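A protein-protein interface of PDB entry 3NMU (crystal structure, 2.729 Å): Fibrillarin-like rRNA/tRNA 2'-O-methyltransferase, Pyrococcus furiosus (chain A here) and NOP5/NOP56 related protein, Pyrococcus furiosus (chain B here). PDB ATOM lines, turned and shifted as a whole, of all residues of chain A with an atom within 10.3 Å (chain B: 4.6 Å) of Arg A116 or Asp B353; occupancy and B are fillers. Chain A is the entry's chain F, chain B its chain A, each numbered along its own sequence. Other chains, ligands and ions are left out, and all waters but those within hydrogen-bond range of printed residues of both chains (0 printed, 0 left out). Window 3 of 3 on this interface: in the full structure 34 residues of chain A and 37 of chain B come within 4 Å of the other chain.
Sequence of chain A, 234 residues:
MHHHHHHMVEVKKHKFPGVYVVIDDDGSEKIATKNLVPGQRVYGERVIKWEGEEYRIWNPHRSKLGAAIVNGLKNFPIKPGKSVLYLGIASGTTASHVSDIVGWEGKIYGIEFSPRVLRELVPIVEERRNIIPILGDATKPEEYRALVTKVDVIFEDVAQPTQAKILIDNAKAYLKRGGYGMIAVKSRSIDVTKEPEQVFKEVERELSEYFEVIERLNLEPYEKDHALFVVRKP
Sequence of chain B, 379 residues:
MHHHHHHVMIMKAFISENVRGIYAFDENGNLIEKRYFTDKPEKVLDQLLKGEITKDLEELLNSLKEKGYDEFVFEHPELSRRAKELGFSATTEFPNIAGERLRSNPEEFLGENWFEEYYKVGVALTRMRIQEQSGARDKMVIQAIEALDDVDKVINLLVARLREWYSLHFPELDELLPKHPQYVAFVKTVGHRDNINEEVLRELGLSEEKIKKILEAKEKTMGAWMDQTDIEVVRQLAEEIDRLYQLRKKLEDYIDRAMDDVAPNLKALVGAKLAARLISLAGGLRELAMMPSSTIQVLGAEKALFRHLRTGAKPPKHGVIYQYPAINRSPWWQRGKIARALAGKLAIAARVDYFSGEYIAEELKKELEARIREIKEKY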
ATOM      1  N   ALA A  90     -12.267  17.902  24.776  1.00  0.00           N
ATOM      2  CA  ALA A  90     -10.975  17.355  25.222  1.00  0.00           C
ATOM      3  C   ALA A  90     -10.344  18.072  26.430  1.00  0.00           C
ATOM      4  O   ALA A  90     -11.049  18.470  27.367  1.00  0.00           O
ATOM      5  CB  ALA A  90      -9.969  17.311  24.043  1.00  0.00           C
ATOM      6  N   SER A  91      -9.021  18.238  26.402  1.00  0.00           N
ATOM      7  CA  SER A  91      -8.327  18.959  27.466  1.00  0.00           C
ATOM      8  C   SER A  91      -8.767  20.413  27.451  1.00  0.00           C
ATOM      9  O   SER A  91      -8.710  21.091  28.473  1.00  0.00           O
ATOM     10  CB  SER A  91      -6.797  18.873  27.313  1.00  0.00           C
ATOM     11  OG  SER A  91      -6.336  17.527  27.341  1.00  0.00           O
ATOM     12  N   GLY A  92      -9.193  20.887  26.277  1.00  0.00           N
ATOM     13  CA  GLY A  92      -9.651  22.256  26.123  1.00  0.00           C
ATOM     14  C   GLY A  92      -8.660  23.198  25.463  1.00  0.00           C
ATOM     15  O   GLY A  92      -8.811  24.423  25.551  1.00  0.00           O
ATOM     16  N   GLU A 112     -17.446  16.082  26.279  1.00  0.00           N
ATOM     17  CA  GLU A 112     -16.273  15.254  26.005  1.00  0.00           C
ATOM     18  C   GLU A 112     -16.465  13.845  26.498  1.00  0.00           C
ATOM     19  O   GLU A 112     -16.724  13.626  27.656  1.00  0.00           O
ATOM     20  CB  GLU A 112     -15.014  15.855  26.626  1.00  0.00           C
ATOM     21  CG  GLU A 112     -13.827  14.902  26.742  1.00  0.00           C
ATOM     22  CD  GLU A 112     -13.338  14.350  25.416  1.00  0.00           C
ATOM     23  OE1 GLU A 112     -12.940  15.134  24.534  1.00  0.00           O
ATOM     24  OE2 GLU A 112     -13.324  13.124  25.253  1.00  0.00           O
ATOM     25  N   PHE A 113     -16.292  12.896  25.594  1.00  0.00           N
ATOM     26  CA  PHE A 113     -16.624  11.505  25.826  1.00  0.00           C
ATOM     27  C   PHE A 113     -15.693  10.745  26.746  1.00  0.00           C
ATOM     28  O   PHE A 113     -16.098   9.734  27.289  1.00  0.00           O
ATOM     29  CB  PHE A 113     -16.653  10.762  24.500  1.00  0.00           C
ATOM     30  CG  PHE A 113     -16.744   9.276  24.650  1.00  0.00           C
ATOM     31  CD1 PHE A 113     -15.600   8.515  24.872  1.00  0.00           C
ATOM     32  CD2 PHE A 113     -17.975   8.632  24.578  1.00  0.00           C
ATOM     33  CE1 PHE A 113     -15.688   7.136  25.022  1.00  0.00           C
ATOM     34  CE2 PHE A 113     -18.065   7.256  24.714  1.00  0.00           C
ATOM     35  CZ  PHE A 113     -16.920   6.507  24.932  1.00  0.00           C
ATOM     36  N   SER A 114     -14.443  11.164  26.888  1.00  0.00           N
ATOM     37  CA  SER A 114     -13.510  10.361  27.655  1.00  0.00           C
ATOM     38  C   SER A 114     -13.003  11.085  28.913  1.00  0.00           C
ATOM     39  O   SER A 114     -12.344  12.122  28.824  1.00  0.00           O
ATOM     40  CB  SER A 114     -12.388   9.841  26.763  1.00  0.00           C
ATOM     41  OG  SER A 114     -11.232   9.525  27.519  1.00  0.00           O
ATOM     42  N   PRO A 115     -13.309  10.524  30.098  1.00  0.00           N
ATOM     43  CA  PRO A 115     -13.250  11.183  31.402  1.00  0.00           C
ATOM     44  C   PRO A 115     -11.873  11.562  31.872  1.00  0.00           C
ATOM     45  O   PRO A 115     -11.760  12.582  32.551  1.00  0.00           O
ATOM     46  CB  PRO A 115     -13.798  10.122  32.357  1.00  0.00           C
ATOM     47  CG  PRO A 115     -14.464   9.124  31.525  1.00  0.00           C
ATOM     48  CD  PRO A 115     -13.740   9.126  30.225  1.00  0.00           C
ATOM     49  N   ARG A 116     -10.857  10.753  31.581  1.00  0.00           N
ATOM     50  CA  ARG A 116      -9.499  11.059  32.053  1.00  0.00           C
ATOM     51  C   ARG A 116      -8.990  12.322  31.386  1.00  0.00           C
ATOM     52  O   ARG A 116      -8.141  13.035  31.923  1.00  0.00           O
ATOM     53  CB  ARG A 116      -8.533   9.911  31.767  1.00  0.00           C
ATOM     54  CG  ARG A 116      -7.113  10.175  32.236  1.00  0.00           C
ATOM     55  CD  ARG A 116      -6.312   8.903  32.196  1.00  0.00           C
ATOM     56  NE  ARG A 116      -6.392   8.285  30.883  1.00  0.00           N
ATOM     57  CZ  ARG A 116      -5.750   7.177  30.533  1.00  0.00           C
ATOM     58  NH1 ARG A 116      -4.975   6.539  31.404  1.00  0.00           N
ATOM     59  NH2 ARG A 116      -5.893   6.706  29.306  1.00  0.00           N
ATOM     60  N   VAL A 117      -9.533  12.575  30.203  1.00  0.00           N
ATOM     61  CA  VAL A 117      -9.221  13.727  29.401  1.00  0.00           C
ATOM     62  C   VAL A 117     -10.052  14.927  29.828  1.00  0.00           C
ATOM     63  O   VAL A 117      -9.489  15.965  30.157  1.00  0.00           O
ATOM     64  CB  VAL A 117      -9.354  13.413  27.931  1.00  0.00           C
ATOM     65  CG1 VAL A 117      -9.433  14.679  27.143  1.00  0.00           C
ATOM     66  CG2 VAL A 117      -8.166  12.571  27.496  1.00  0.00           C
ATOM     67  N   LEU A 118     -11.376  14.827  29.804  1.00  0.00           N
ATOM     68  CA  LEU A 118     -12.164  15.969  30.264  1.00  0.00           C
ATOM     69  C   LEU A 118     -11.657  16.443  31.625  1.00  0.00           C
ATOM     70  O   LEU A 118     -11.717  17.628  31.937  1.00  0.00           O
ATOM     71  CB  LEU A 118     -13.668  15.664  30.340  1.00  0.00           C
ATOM     72  CG  LEU A 118     -14.601  16.759  30.892  1.00  0.00           C
ATOM     73  CD1 LEU A 118     -14.468  18.039  30.155  1.00  0.00           C
ATOM     74  CD2 LEU A 118     -16.029  16.336  30.803  1.00  0.00           C
ATOM     75  N   ARG A 119     -11.116  15.530  32.423  1.00  0.00           N
ATOM     76  CA  ARG A 119     -10.678  15.886  33.773  1.00  0.00           C
ATOM     77  C   ARG A 119      -9.672  17.038  33.769  1.00  0.00           C
ATOM     78  O   ARG A 119      -9.779  17.971  34.577  1.00  0.00           O
ATOM     79  CB  ARG A 119     -10.116  14.670  34.514  1.00  0.00           C
ATOM     80  CG  ARG A 119     -10.117  14.842  36.037  1.00  0.00           C
ATOM     81  CD  ARG A 119      -9.843  13.543  36.758  1.00  0.00           C
ATOM     82  NE  ARG A 119      -8.532  13.018  36.402  1.00  0.00           N
ATOM     83  CZ  ARG A 119      -8.317  11.774  35.993  1.00  0.00           C
ATOM     84  NH1 ARG A 119      -7.091  11.371  35.692  1.00  0.00           N
ATOM     85  NH2 ARG A 119      -9.333  10.931  35.896  1.00  0.00           N
ATOM     86  N   GLU A 120      -8.713  16.984  32.845  1.00  0.00           N
ATOM     87  CA  GLU A 120      -7.730  18.053  32.709  1.00  0.00           C
ATOM     88  C   GLU A 120      -8.402  19.409  32.611  1.00  0.00           C
ATOM     89  O   GLU A 120      -7.875  20.401  33.097  1.00  0.00           O
ATOM     90  CB  GLU A 120      -6.884  17.840  31.471  1.00  0.00           C
ATOM     91  CG  GLU A 120      -6.528  16.405  31.227  1.00  0.00           C
ATOM     92  CD  GLU A 120      -5.423  15.932  32.137  1.00  0.00           C
ATOM     93  OE1 GLU A 120      -5.122  14.719  32.092  1.00  0.00           O
ATOM     94  OE2 GLU A 120      -4.854  16.769  32.886  1.00  0.00           O
ATOM     95  N   LEU A 121      -9.569  19.442  31.980  1.00  0.00           N
ATOM     96  CA  LEU A 121     -10.255  20.699  31.688  1.00  0.00           C
ATOM     97  C   LEU A 121     -10.984  21.249  32.891  1.00  0.00           C
ATOM     98  O   LEU A 121     -11.156  22.461  33.015  1.00  0.00           O
ATOM     99  CB  LEU A 121     -11.246  20.513  30.530  1.00  0.00           C
ATOM    100  CG  LEU A 121     -12.257  21.612  30.198  1.00  0.00           C
ATOM    101  CD1 LEU A 121     -11.557  22.861  29.745  1.00  0.00           C
ATOM    102  CD2 LEU A 121     -13.192  21.129  29.119  1.00  0.00           C
ATOM    103  N   VAL A 122     -11.407  20.354  33.779  1.00  0.00           N
ATOM    104  CA  VAL A 122     -12.322  20.723  34.858  1.00  0.00           C
ATOM    105  C   VAL A 122     -11.794  21.825  35.785  1.00  0.00           C
ATOM    106  O   VAL A 122     -12.467  22.846  35.971  1.00  0.00           O
ATOM    107  CB  VAL A 122     -12.778  19.493  35.673  1.00  0.00           C
ATOM    108  CG1 VAL A 122     -13.953  19.856  36.563  1.00  0.00           C
ATOM    109  CG2 VAL A 122     -13.170  18.368  34.736  1.00  0.00           C
ATOM    110  N   PRO A 123     -10.585  21.641  36.345  1.00  0.00           N
ATOM    111  CA  PRO A 123     -10.006  22.602  37.290  1.00  0.00           C
ATOM    112  C   PRO A 123      -9.752  23.955  36.647  1.00  0.00           C
ATOM    113  O   PRO A 123      -9.558  24.965  37.335  1.00  0.00           O
ATOM    114  CB  PRO A 123      -8.666  21.959  37.648  1.00  0.00           C
ATOM    115  CG  PRO A 123      -8.314  21.161  36.470  1.00  0.00           C
ATOM    116  CD  PRO A 123      -9.627  20.575  36.012  1.00  0.00           C
ATOM    117  N   LEU A 135     -19.344  15.676  30.866  1.00  0.00           N
ATOM    118  CA  LEU A 135     -19.026  14.357  30.332  1.00  0.00           C
ATOM    119  C   LEU A 135     -20.239  13.811  29.563  1.00  0.00           C
ATOM    120  O   LEU A 135     -21.365  13.803  30.059  1.00  0.00           O
ATOM    121  CB  LEU A 135     -18.551  13.409  31.424  1.00  0.00           C
ATOM    122  CG  LEU A 135     -18.161  11.992  30.989  1.00  0.00           C
ATOM    123  CD1 LEU A 135     -16.759  11.925  30.428  1.00  0.00           C
ATOM    124  CD2 LEU A 135     -18.282  11.011  32.176  1.00  0.00           C
ATOM    125  N   GLY A 136     -20.011  13.384  28.333  1.00  0.00           N
ATOM    126  CA  GLY A 136     -21.103  12.952  27.488  1.00  0.00           C
ATOM    127  C   GLY A 136     -20.641  12.343  26.177  1.00  0.00           C
ATOM    128  O   GLY A 136     -19.449  12.330  25.877  1.00  0.00           O
ATOM    129  N   ASP B 261     -11.763   5.072  32.822  1.00  0.00           N
ATOM    130  CA  ASP B 261     -10.627   5.882  33.235  1.00  0.00           C
ATOM    131  C   ASP B 261      -9.284   5.239  32.905  1.00  0.00           C
ATOM    132  O   ASP B 261      -8.222   5.762  33.259  1.00  0.00           O
ATOM    133  CB  ASP B 261     -10.729   6.206  34.721  1.00  0.00           C
ATOM    134  CG  ASP B 261      -9.774   7.311  35.149  1.00  0.00           C
ATOM    135  OD1 ASP B 261      -8.614   7.014  35.569  1.00  0.00           O
ATOM    136  OD2 ASP B 261     -10.212   8.480  35.076  1.00  0.00           O
ATOM    137  N   VAL B 262      -9.325   4.083  32.263  1.00  0.00           N
ATOM    138  CA  VAL B 262      -8.126   3.256  32.146  1.00  0.00           C
ATOM    139  C   VAL B 262      -7.810   2.953  30.709  1.00  0.00           C
ATOM    140  O   VAL B 262      -6.720   3.227  30.229  1.00  0.00           O
ATOM    141  CB  VAL B 262      -8.236   1.936  32.959  1.00  0.00           C
ATOM    142  CG1 VAL B 262      -7.138   0.959  32.562  1.00  0.00           C
ATOM    143  CG2 VAL B 262      -8.137   2.231  34.430  1.00  0.00           C
ATOM    144  N   ALA B 263      -8.754   2.314  30.043  1.00  0.00           N
ATOM    145  CA  ALA B 263      -8.619   2.046  28.631  1.00  0.00           C
ATOM    146  C   ALA B 263      -9.951   2.159  27.895  1.00  0.00           C
ATOM    147  O   ALA B 263     -10.453   1.163  27.391  1.00  0.00           O
ATOM    148  CB  ALA B 263      -7.983   0.676  28.413  1.00  0.00           C
ATOM    149  N   PRO B 264     -10.502   3.384  27.787  1.00  0.00           N
ATOM    150  CA  PRO B 264     -11.787   3.559  27.104  1.00  0.00           C
ATOM    151  C   PRO B 264     -11.754   2.900  25.736  1.00  0.00           C
ATOM    152  O   PRO B 264     -12.737   2.262  25.325  1.00  0.00           O
ATOM    153  CB  PRO B 264     -11.898   5.074  26.933  1.00  0.00           C
ATOM    154  CG  PRO B 264     -10.954   5.659  27.890  1.00  0.00           C
ATOM    155  CD  PRO B 264      -9.845   4.674  28.057  1.00  0.00           C
ATOM    156  N   ASN B 265     -10.626   3.048  25.045  1.00  0.00           N
ATOM    157  CA  ASN B 265     -10.478   2.470  23.711  1.00  0.00           C
ATOM    158  C   ASN B 265     -10.523   0.975  23.756  1.00  0.00           C
ATOM    159  O   ASN B 265     -11.267   0.357  22.992  1.00  0.00           O
ATOM    160  CB  ASN B 265      -9.171   2.895  23.038  1.00  0.00           C
ATOM    161  CG  ASN B 265      -9.218   4.299  22.571  1.00  0.00           C
ATOM    162  OD1 ASN B 265     -10.081   4.662  21.777  1.00  0.00           O
ATOM    163  ND2 ASN B 265      -8.325   5.127  23.095  1.00  0.00           N
ATOM    164  N   LEU B 266      -9.702   0.405  24.635  1.00  0.00           N
ATOM    165  CA  LEU B 266      -9.686  -1.036  24.846  1.00  0.00           C
ATOM    166  C   LEU B 266     -11.062  -1.557  25.234  1.00  0.00           C
ATOM    167  O   LEU B 266     -11.531  -2.561  24.708  1.00  0.00           O
ATOM    168  CB  LEU B 266      -8.648  -1.398  25.886  1.00  0.00           C
ATOM    169  CG  LEU B 266      -7.311  -1.623  25.208  1.00  0.00           C
ATOM    170  CD1 LEU B 266      -6.227  -1.843  26.207  1.00  0.00           C
ATOM    171  CD2 LEU B 266      -7.484  -2.826  24.331  1.00  0.00           C
ATOM    172  N   LEU B 285      -1.310  -1.340  32.272  1.00  0.00           N
ATOM    173  CA  LEU B 285      -1.739  -0.756  31.015  1.00  0.00           C
ATOM    174  C   LEU B 285      -0.473  -0.416  30.245  1.00  0.00           C
ATOM    175  O   LEU B 285      -0.409  -0.557  29.032  1.00  0.00           O
ATOM    176  CB  LEU B 285      -2.624   0.466  31.286  1.00  0.00           C
ATOM    177  CG  LEU B 285      -2.984   1.501  30.225  1.00  0.00           C
ATOM    178  CD1 LEU B 285      -3.669   0.884  29.033  1.00  0.00           C
ATOM    179  CD2 LEU B 285      -3.865   2.567  30.873  1.00  0.00           C
ATOM    180  N   ALA B 349      -5.054   0.751  20.414  1.00  0.00           N
ATOM    181  CA  ALA B 349      -6.005   1.206  21.412  1.00  0.00           C
ATOM    182  C   ALA B 349      -5.274   1.278  22.743  1.00  0.00           C
ATOM    183  O   ALA B 349      -5.421   2.238  23.494  1.00  0.00           O
ATOM    184  CB  ALA B 349      -7.179   0.297  21.479  1.00  0.00           C
ATOM    185  N   ALA B 350      -4.434   0.287  23.006  1.00  0.00           N
ATOM    186  CA  ALA B 350      -3.681   0.247  24.253  1.00  0.00           C
ATOM    187  C   ALA B 350      -2.705   1.429  24.390  1.00  0.00           C
ATOM    188  O   ALA B 350      -2.580   2.036  25.464  1.00  0.00           O
ATOM    189  CB  ALA B 350      -2.941  -1.059  24.349  1.00  0.00           C
ATOM    190  N   ARG B 351      -2.013   1.752  23.296  1.00  0.00           N
ATOM    191  CA  ARG B 351      -1.067   2.857  23.308  1.00  0.00           C
ATOM    192  C   ARG B 351      -1.786   4.201  23.360  1.00  0.00           C
ATOM    193  O   ARG B 351      -1.323   5.110  24.046  1.00  0.00           O
ATOM    194  CB  ARG B 351      -0.109   2.766  22.126  1.00  0.00           C
ATOM    195  CG  ARG B 351       0.405   1.363  21.890  1.00  0.00           C
ATOM    196  CD  ARG B 351       1.784   1.347  21.295  1.00  0.00           C
ATOM    197  NE  ARG B 351       1.813   0.724  19.976  1.00  0.00           N
ATOM    198  CZ  ARG B 351       2.310  -0.483  19.741  1.00  0.00           C
ATOM    199  NH1 ARG B 351       2.793  -1.173  20.751  1.00  0.00           N
ATOM    200  NH2 ARG B 351       2.323  -1.007  18.519  1.00  0.00           N
ATOM    201  N   VAL B 352      -2.929   4.330  22.680  1.00  0.00           N
ATOM    202  CA  VAL B 352      -3.708   5.563  22.825  1.00  0.00           C
ATOM    203  C   VAL B 352      -4.181   5.706  24.262  1.00  0.00           C
ATOM    204  O   VAL B 352      -3.957   6.733  24.905  1.00  0.00           O
ATOM    205  CB  VAL B 352      -4.922   5.640  21.914  1.00  0.00           C
ATOM    206  CG1 VAL B 352      -5.593   6.986  22.089  1.00  0.00           C
ATOM    207  CG2 VAL B 352      -4.520   5.440  20.464  1.00  0.00           C
ATOM    208  N   ASP B 353      -4.828   4.653  24.755  1.00  0.00           N
ATOM    209  CA  ASP B 353      -5.249   4.568  26.141  1.00  0.00           C
ATOM    210  C   ASP B 353      -4.131   4.914  27.121  1.00  0.00           C
ATOM    211  O   ASP B 353      -4.314   5.721  28.030  1.00  0.00           O
ATOM    212  CB  ASP B 353      -5.775   3.163  26.436  1.00  0.00           C
ATOM    213  CG  ASP B 353      -7.233   2.972  26.019  1.00  0.00           C
ATOM    214  OD1 ASP B 353      -8.016   3.949  26.069  1.00  0.00           O
ATOM    215  OD2 ASP B 353      -7.612   1.829  25.658  1.00  0.00           O
ATOM    216  N   TYR B 354      -2.962   4.314  26.956  1.00  0.00           N
ATOM    217  CA  TYR B 354      -1.899   4.617  27.909  1.00  0.00           C
ATOM    218  C   TYR B 354      -1.485   6.097  27.914  1.00  0.00           C
ATOM    219  O   TYR B 354      -1.324   6.687  28.977  1.00  0.00           O
ATOM    220  CB  TYR B 354      -0.666   3.745  27.688  1.00  0.00           C
ATOM    221  CG  TYR B 354       0.389   4.054  28.704  1.00  0.00           C
ATOM    222  CD1 TYR B 354       0.178   3.781  30.050  1.00  0.00           C
ATOM    223  CD2 TYR B 354       1.579   4.634  28.341  1.00  0.00           C
ATOM    224  CE1 TYR B 354       1.130   4.065  31.003  1.00  0.00           C
ATOM    225  CE2 TYR B 354       2.548   4.930  29.283  1.00  0.00           C
ATOM    226  CZ  TYR B 354       2.320   4.640  30.618  1.00  0.00           C
ATOM    227  OH  TYR B 354       3.280   4.940  31.565  1.00  0.00           O
ATOM    228  N   PHE B 355      -1.287   6.662  26.711  1.00  0.00           N
ATOM    229  CA  PHE B 355      -0.718   8.013  26.507  1.00  0.00           C
ATOM    230  C   PHE B 355      -1.629   9.245  26.582  1.00  0.00           C
ATOM    231  O   PHE B 355      -1.270  10.240  27.213  1.00  0.00           O
ATOM    232  CB  PHE B 355       0.094   8.053  25.212  1.00  0.00           C
ATOM    233  CG  PHE B 355       1.349   7.245  25.283  1.00  0.00           C
ATOM    234  CD1 PHE B 355       2.380   7.621  26.141  1.00  0.00           C
ATOM    235  CD2 PHE B 355       1.498   6.103  24.515  1.00  0.00           C
ATOM    236  CE1 PHE B 355       3.549   6.868  26.231  1.00  0.00           C
ATOM    237  CE2 PHE B 355       2.647   5.344  24.588  1.00  0.00           C
ATOM    238  CZ  PHE B 355       3.680   5.721  25.455  1.00  0.00           C
ATOM    239  N   SER B 356      -2.790   9.179  25.942  1.00  0.00           N
ATOM    240  CA  SER B 356      -3.730  10.299  25.927  1.00  0.00           C
ATOM    241  C   SER B 356      -5.067   9.922  26.557  1.00  0.00           C
ATOM    242  O   SER B 356      -5.538  10.584  27.480  1.00  0.00           O
ATOM    243  CB  SER B 356      -3.907  10.893  24.518  1.00  0.00           C
ATOM    244  OG  SER B 356      -4.390   9.950  23.584  1.00  0.00           O
ATOM    245  N   GLY B 357      -5.700   8.893  26.006  1.00  0.00           N
ATOM    246  CA  GLY B 357      -6.997   8.443  26.475  1.00  0.00           C
ATOM    247  C   GLY B 357      -8.103   9.041  25.631  1.00  0.00           C
ATOM    248  O   GLY B 357      -9.273   8.983  25.984  1.00  0.00           O
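Gly A92 touches none of the printed residues of chain B. Printed residues of chain B within 4 Å of Ser A114: Pro B264 (3.9 Å) and Gly B357 (2.5 Å). Arg A116 touches four residues of chain B. Printed residues of chain B within 4 Å of Arg A119: Asp B261. Of the printed residues of chain A, Asp B261 touches Arg A116 and Arg A119. Val B262 touches just one residue of chain A: Arg A116. No residue of chain A comes within 4 Å of Ala B263. Of the printed residues of chain A, Pro B264 touches Ser A114. No residue of chain A comes within 4 Å of Asn B265. No residue of chain A comes within 4 Å of Leu B266. No residue of chain A comes within 4 Å of Ala B350. No residue of chain A comes within 4 Å of Val B352. Of chain A, only Arg A116 comes within 4 Å of Asp B353. Tyr B354 touches none of the printed residues of chain A. Of the printed residues of chain A, Ser B356 touches Val A117. Printed residues of chain A within 4 Å of Gly B357: Ser A114 (2.5 Å), Arg A116 (3.5 Å) and Val A117 (3.99 Å).
The backbone NH (N) of Asn B265 lies within hydrogen-bond range of the side-chain carboxylate (OD1) of Asp B353, 2.9 Å away. The backbone NH of Leu B266 lies within hydrogen-bond range of the side-chain carboxylate of Asp B353 (2.7 Å). N of Gly B357 is in hydrogen-bond range of O of Val B352 (3.0 Å). The side-chain carboxylate (OE2) of Glu A112 is in hydrogen-bond range of the backbone NH (N) of Ser A114 (2.8 Å).
Ser A114 touches Pro B264. NH1 of Arg A116 touches O of Asp B261, at 3.8 Å. O of Val B262 touches NH2 of Arg A116 (3.7 Å). CA of Gly B357 touches NH2 of Arg A116, 3.5 Å away. CG2 of Val A117 touches O of Ser B356, 3.3 Å away. Gly B357 touches Val A117.
Of the 16 printed residues of chain B, 6 touch a printed residue of chain A. Of the 17 printed residues of chain A, 4 touch a printed residue of chain B. Printed residues of chain A that touch a printed residue of chain B: Ser A114, Arg A116, Val A117 and Arg A119. Hydrophobic or aromatic side chains of chain A that line the printed part of chain B: Val A117.
The side-chain carboxylate of Asp B261 lies within salt-bridge range of the guanidinium group of Arg A119. O of Gly B357 sits at hydrogen-bond distance from OG of Ser A114 (2.5 Å). O of Asp B353 sits close to NH2 of Arg A116 (2.3 Å).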
